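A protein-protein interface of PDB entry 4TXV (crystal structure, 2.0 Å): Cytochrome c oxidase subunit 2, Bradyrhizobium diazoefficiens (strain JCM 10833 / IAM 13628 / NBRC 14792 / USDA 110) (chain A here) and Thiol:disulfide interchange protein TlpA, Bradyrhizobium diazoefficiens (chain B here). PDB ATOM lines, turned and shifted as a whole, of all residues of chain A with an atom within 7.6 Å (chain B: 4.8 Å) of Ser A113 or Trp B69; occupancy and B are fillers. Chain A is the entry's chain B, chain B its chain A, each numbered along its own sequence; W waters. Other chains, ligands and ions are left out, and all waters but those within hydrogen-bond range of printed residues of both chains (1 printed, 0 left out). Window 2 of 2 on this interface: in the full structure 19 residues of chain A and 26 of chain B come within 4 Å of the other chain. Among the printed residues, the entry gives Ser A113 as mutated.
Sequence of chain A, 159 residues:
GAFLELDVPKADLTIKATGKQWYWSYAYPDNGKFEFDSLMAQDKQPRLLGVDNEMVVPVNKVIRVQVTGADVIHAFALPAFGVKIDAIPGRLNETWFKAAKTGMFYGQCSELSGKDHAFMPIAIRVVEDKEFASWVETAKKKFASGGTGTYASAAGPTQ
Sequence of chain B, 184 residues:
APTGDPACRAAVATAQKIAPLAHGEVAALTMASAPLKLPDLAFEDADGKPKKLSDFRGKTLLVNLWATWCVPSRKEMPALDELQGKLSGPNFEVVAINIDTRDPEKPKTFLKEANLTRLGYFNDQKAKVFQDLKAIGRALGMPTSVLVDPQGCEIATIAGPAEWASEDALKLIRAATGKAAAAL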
ATOM      1  N   CYS A 109      13.935  12.691  -3.141  1.00  0.00           N
ATOM      2  CA  CYS A 109      15.099  13.117  -2.346  1.00  0.00           C
ATOM      3  C   CYS A 109      15.271  12.204  -1.121  1.00  0.00           C
ATOM      4  O   CYS A 109      14.289  11.719  -0.544  1.00  0.00           O
ATOM      5  CB  CYS A 109      14.908  14.504  -1.725  1.00  0.00           C
ATOM      6  SG  CYS A 109      14.541  15.721  -2.941  1.00  0.00           S
ATOM      7  N   SER A 110      16.489  12.055  -0.645  1.00  0.00           N
ATOM      8  CA  SER A 110      16.671  11.265   0.573  1.00  0.00           C
ATOM      9  C   SER A 110      16.080  12.084   1.714  1.00  0.00           C
ATOM     10  O   SER A 110      15.817  13.277   1.576  1.00  0.00           O
ATOM     11  CB  SER A 110      18.134  10.955   0.839  1.00  0.00           C
ATOM     12  OG  SER A 110      18.776  12.168   1.074  1.00  0.00           O
ATOM     13  N   GLU A 111      15.837  11.442   2.837  1.00  0.00           N
ATOM     14  CA  GLU A 111      15.204  12.136   3.943  1.00  0.00           C
ATOM     15  C   GLU A 111      16.122  13.221   4.557  1.00  0.00           C
ATOM     16  O   GLU A 111      15.621  14.203   5.100  1.00  0.00           O
ATOM     17  CB  GLU A 111      14.753  11.125   4.979  1.00  0.00           C
ATOM     18  CG  GLU A 111      15.847  10.214   5.510  1.00  0.00           C
ATOM     19  CD  GLU A 111      15.394   9.471   6.748  1.00  0.00           C
ATOM     20  OE1 GLU A 111      15.350   8.232   6.662  1.00  0.00           O
ATOM     21  OE2 GLU A 111      15.053  10.120   7.783  1.00  0.00           O
ATOM     22  N   LEU A 112      17.448  13.033   4.457  1.00  0.00           N
ATOM     23  CA  LEU A 112      18.452  14.086   4.756  1.00  0.00           C
ATOM     24  C   LEU A 112      18.224  15.340   3.877  1.00  0.00           C
ATOM     25  O   LEU A 112      18.173  15.228   2.642  1.00  0.00           O
ATOM     26  CB  LEU A 112      19.903  13.541   4.521  1.00  0.00           C
ATOM     27  CG  LEU A 112      20.495  13.302   3.076  1.00  0.00           C
ATOM     28  CD1 LEU A 112      21.427  14.417   2.550  1.00  0.00           C
ATOM     29  CD2 LEU A 112      21.184  11.933   2.897  1.00  0.00           C
ATOM     30  N   SER A 113      18.093  16.532   4.456  1.00  0.00           N
ATOM     31  CA  SER A 113      18.222  17.719   3.599  1.00  0.00           C
ATOM     32  C   SER A 113      19.593  17.696   2.860  1.00  0.00           C
ATOM     33  O   SER A 113      20.650  17.466   3.466  1.00  0.00           O
ATOM     34  CB  SER A 113      18.061  19.009   4.384  1.00  0.00           C
ATOM     35  OG  SER A 113      18.319  20.113   3.521  1.00  0.00           O
ATOM     36  N   GLY A 114      19.566  17.889   1.547  1.00  0.00           N
ATOM     37  CA  GLY A 114      20.786  17.857   0.746  1.00  0.00           C
ATOM     38  C   GLY A 114      20.908  19.157  -0.018  1.00  0.00           C
ATOM     39  O   GLY A 114      19.966  19.953  -0.076  1.00  0.00           O
ATOM     40  N   LYS A 115      22.049  19.353  -0.664  1.00  0.00           N
ATOM     41  CA  LYS A 115      22.381  20.675  -1.183  1.00  0.00           C
ATOM     42  C   LYS A 115      22.417  20.865  -2.718  1.00  0.00           C
ATOM     43  O   LYS A 115      22.892  20.027  -3.462  1.00  0.00           O
ATOM     44  CB  LYS A 115      23.695  21.207  -0.553  1.00  0.00           C
ATOM     45  CG  LYS A 115      24.727  20.179  -0.112  1.00  0.00           C
ATOM     46  CD  LYS A 115      25.903  20.059  -1.076  1.00  0.00           C
ATOM     47  CE  LYS A 115      27.063  19.337  -0.404  1.00  0.00           C
ATOM     48  NZ  LYS A 115      27.307  19.841   0.984  1.00  0.00           N
ATOM     49  N   ASP A 116      21.791  21.965  -3.140  1.00  0.00           N
ATOM     50  CA  ASP A 116      22.386  22.974  -4.060  1.00  0.00           C
ATOM     51  C   ASP A 116      22.686  22.594  -5.496  1.00  0.00           C
ATOM     52  O   ASP A 116      23.851  22.362  -5.836  1.00  0.00           O
ATOM     53  CB  ASP A 116      23.663  23.527  -3.420  1.00  0.00           C
ATOM     54  CG  ASP A 116      23.396  24.204  -2.045  1.00  0.00           C
ATOM     55  OD1 ASP A 116      22.319  23.982  -1.392  1.00  0.00           O
ATOM     56  OD2 ASP A 116      24.281  24.978  -1.609  1.00  0.00           O
ATOM     57  N   PHE A 119      20.137  17.994  -6.983  1.00  0.00           N
ATOM     58  CA  PHE A 119      19.052  17.003  -7.256  1.00  0.00           C
ATOM     59  C   PHE A 119      19.167  16.379  -8.649  1.00  0.00           C
ATOM     60  O   PHE A 119      19.123  17.093  -9.631  1.00  0.00           O
ATOM     61  CB  PHE A 119      17.665  17.609  -7.156  1.00  0.00           C
ATOM     62  CG  PHE A 119      16.572  16.570  -7.280  1.00  0.00           C
ATOM     63  CD1 PHE A 119      16.402  15.627  -6.295  1.00  0.00           C
ATOM     64  CD2 PHE A 119      15.798  16.500  -8.395  1.00  0.00           C
ATOM     65  CE1 PHE A 119      15.434  14.640  -6.440  1.00  0.00           C
ATOM     66  CE2 PHE A 119      14.810  15.550  -8.533  1.00  0.00           C
ATOM     67  CZ  PHE A 119      14.639  14.621  -7.567  1.00  0.00           C
ATOM     68  N   ALA B  67       8.560  19.684   1.622  1.00  0.00           N
ATOM     69  CA  ALA B  67       9.537  20.547   2.238  1.00  0.00           C
ATOM     70  C   ALA B  67      10.183  21.421   1.184  1.00  0.00           C
ATOM     71  O   ALA B  67      10.384  20.971   0.063  1.00  0.00           O
ATOM     72  CB  ALA B  67      10.587  19.696   2.904  1.00  0.00           C
ATOM     73  N   THR B  68      10.615  22.635   1.546  1.00  0.00           N
ATOM     74  CA  THR B  68      11.156  23.565   0.523  1.00  0.00           C
ATOM     75  C   THR B  68      12.504  23.133   0.094  1.00  0.00           C
ATOM     76  O   THR B  68      12.967  23.581  -0.936  1.00  0.00           O
ATOM     77  CB  THR B  68      11.321  25.009   1.034  1.00  0.00           C
ATOM     78  OG1 THR B  68      12.258  25.011   2.104  1.00  0.00           O
ATOM     79  CG2 THR B  68      10.011  25.546   1.533  1.00  0.00           C
ATOM     80  N   TRP B  69      13.157  22.244   0.850  1.00  0.00           N
ATOM     81  CA  TRP B  69      14.488  21.810   0.471  1.00  0.00           C
ATOM     82  C   TRP B  69      14.448  20.634  -0.498  1.00  0.00           C
ATOM     83  O   TRP B  69      15.493  20.242  -1.038  1.00  0.00           O
ATOM     84  CB  TRP B  69      15.307  21.449   1.698  1.00  0.00           C
ATOM     85  CG  TRP B  69      14.660  20.448   2.650  1.00  0.00           C
ATOM     86  CD1 TRP B  69      14.023  20.726   3.820  1.00  0.00           C
ATOM     87  CD2 TRP B  69      14.599  19.009   2.492  1.00  0.00           C
ATOM     88  NE1 TRP B  69      13.538  19.558   4.383  1.00  0.00           N
ATOM     89  CE2 TRP B  69      13.914  18.493   3.604  1.00  0.00           C
ATOM     90  CE3 TRP B  69      15.088  18.118   1.528  1.00  0.00           C
ATOM     91  CZ2 TRP B  69      13.667  17.126   3.767  1.00  0.00           C
ATOM     92  CZ3 TRP B  69      14.846  16.750   1.700  1.00  0.00           C
ATOM     93  CH2 TRP B  69      14.139  16.278   2.809  1.00  0.00           C
ATOM     94  N   CYS B  70      13.264  20.063  -0.721  1.00  0.00           N
ATOM     95  CA  CYS B  70      13.108  18.916  -1.640  1.00  0.00           C
ATOM     96  C   CYS B  70      12.453  19.351  -2.942  1.00  0.00           C
ATOM     97  O   CYS B  70      11.269  19.703  -2.970  1.00  0.00           O
ATOM     98  CB  CYS B  70      12.284  17.834  -0.953  1.00  0.00           C
ATOM     99  SG  CYS B  70      11.832  16.490  -2.061  1.00  0.00           S
ATOM    100  N   VAL B  71      13.213  19.335  -4.014  1.00  0.00           N
ATOM    101  CA  VAL B  71      12.746  19.841  -5.273  1.00  0.00           C
ATOM    102  C   VAL B  71      11.479  19.149  -5.841  1.00  0.00           C
ATOM    103  O   VAL B  71      10.512  19.860  -6.233  1.00  0.00           O
ATOM    104  CB  VAL B  71      13.889  19.787  -6.276  1.00  0.00           C
ATOM    105  CG1 VAL B  71      13.406  19.995  -7.716  1.00  0.00           C
ATOM    106  CG2 VAL B  71      14.997  20.822  -5.888  1.00  0.00           C
ATOM    107  N   ARG B  74       8.490  20.258  -3.885  1.00  0.00           N
ATOM    108  CA  ARG B  74       8.067  21.611  -4.291  1.00  0.00           C
ATOM    109  C   ARG B  74       7.301  21.618  -5.598  1.00  0.00           C
ATOM    110  O   ARG B  74       6.215  22.247  -5.725  1.00  0.00           O
ATOM    111  CB  ARG B  74       9.251  22.557  -4.502  1.00  0.00           C
ATOM    112  CG  ARG B  74       9.991  22.989  -3.239  1.00  0.00           C
ATOM    113  CD  ARG B  74      10.735  24.322  -3.438  1.00  0.00           C
ATOM    114  NE  ARG B  74      11.547  24.396  -4.639  1.00  0.00           N
ATOM    115  CZ  ARG B  74      12.827  24.014  -4.712  1.00  0.00           C
ATOM    116  NH1 ARG B  74      13.482  24.133  -5.862  1.00  0.00           N
ATOM    117  NH2 ARG B  74      13.480  23.516  -3.645  1.00  0.00           N
ATOM    118  N   ASP B 100       9.448  21.535   6.970  1.00  0.00           N
ATOM    119  CA  ASP B 100      10.688  22.267   7.117  1.00  0.00           C
ATOM    120  C   ASP B 100      10.946  22.422   8.610  1.00  0.00           C
ATOM    121  O   ASP B 100      10.023  22.682   9.395  1.00  0.00           O
ATOM    122  CB  ASP B 100      10.642  23.660   6.496  1.00  0.00           C
ATOM    123  CG  ASP B 100      10.756  23.626   5.001  1.00  0.00           C
ATOM    124  OD1 ASP B 100       9.950  22.902   4.402  1.00  0.00           O
ATOM    125  OD2 ASP B 100      11.590  24.330   4.418  1.00  0.00           O
ATOM    126  N   MET B 142      11.543  11.897   0.355  1.00  0.00           N
ATOM    127  CA  MET B 142      10.604  12.946   0.076  1.00  0.00           C
ATOM    128  C   MET B 142      10.414  13.221  -1.406  1.00  0.00           C
ATOM    129  O   MET B 142      11.385  13.177  -2.203  1.00  0.00           O
ATOM    130  CB  MET B 142      11.137  14.206   0.775  1.00  0.00           C
ATOM    131  CG  MET B 142      10.976  14.184   2.289  1.00  0.00           C
ATOM    132  SD  MET B 142       9.272  14.263   2.836  1.00  0.00           S
ATOM    133  CE  MET B 142       8.895  16.008   2.578  1.00  0.00           C
HETATM  134  O   HOH W   1      15.981  18.613  -3.657  1.00  0.00           O
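SG of Cys A109 touches N of Val B71, 3.997 Å away.
CZ3 of Trp B69 touches O of Ser A110, at 3.6 Å.
Trp B69 touches Glu A111 (CH2 to O, 3.4 Å).
Leu A112 touches Trp B69.
CB of Trp B69 touches OG of Ser A113, at 3.8 Å.
The side-chain hydroxyl (OG) of Ser A110 sits close to the backbone carbonyl oxygen (O) of Leu A112 (3.5 Å).
The side-chain sulfur (SG) of Cys B70 lies within hydrogen-bond range of the backbone carbonyl oxygen (O) of Met B142 (3.3 Å).
Water W1 lies within hydrogen-bond range of the backbone NH of Val B71 (2.9 Å), the backbone carbonyl oxygen of Trp B69 (3.1 Å) and the side-chain sulfur of Cys A109 (3.3 Å).
Of the 8 printed residues of chain B, 4 touch a printed residue of chain A.
Hydrophobic or aromatic side chains of chain B that line the printed part of chain A: Trp B69.
Of chain B, only Trp B69 comes within 4 Å of Ser A113.
Printed residues of chain A within 4 Å of Trp B69: Ser A110 (3.6 Å), Glu A111 (3.4 Å), Leu A112 (3.8 Å) and Ser A113 (3.8 Å).
Printed residues of chain B within 4 Å of Glu A111: Trp B69.
Printed residues of chain A within 4 Å of Val B71: Cys A109.
The nearest printed residue of chain B that does not touch Ser A113 is Cys B70 (6.6 Å).
The nearest residue of chain A that does not touch Trp B69 is Cys A109 (4.1 Å).
The nearest printed residue of chain A that does not touch Cys B70 is Phe A119 (6.0 Å).
The side-chain sulfur (SG) of Cys B70 sits close to the side-chain sulfur (SG) of Cys A109 (3.0 Å).
N of Cys A109 lies within hydrogen-bond range of O of Met B142 (2.8 Å).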
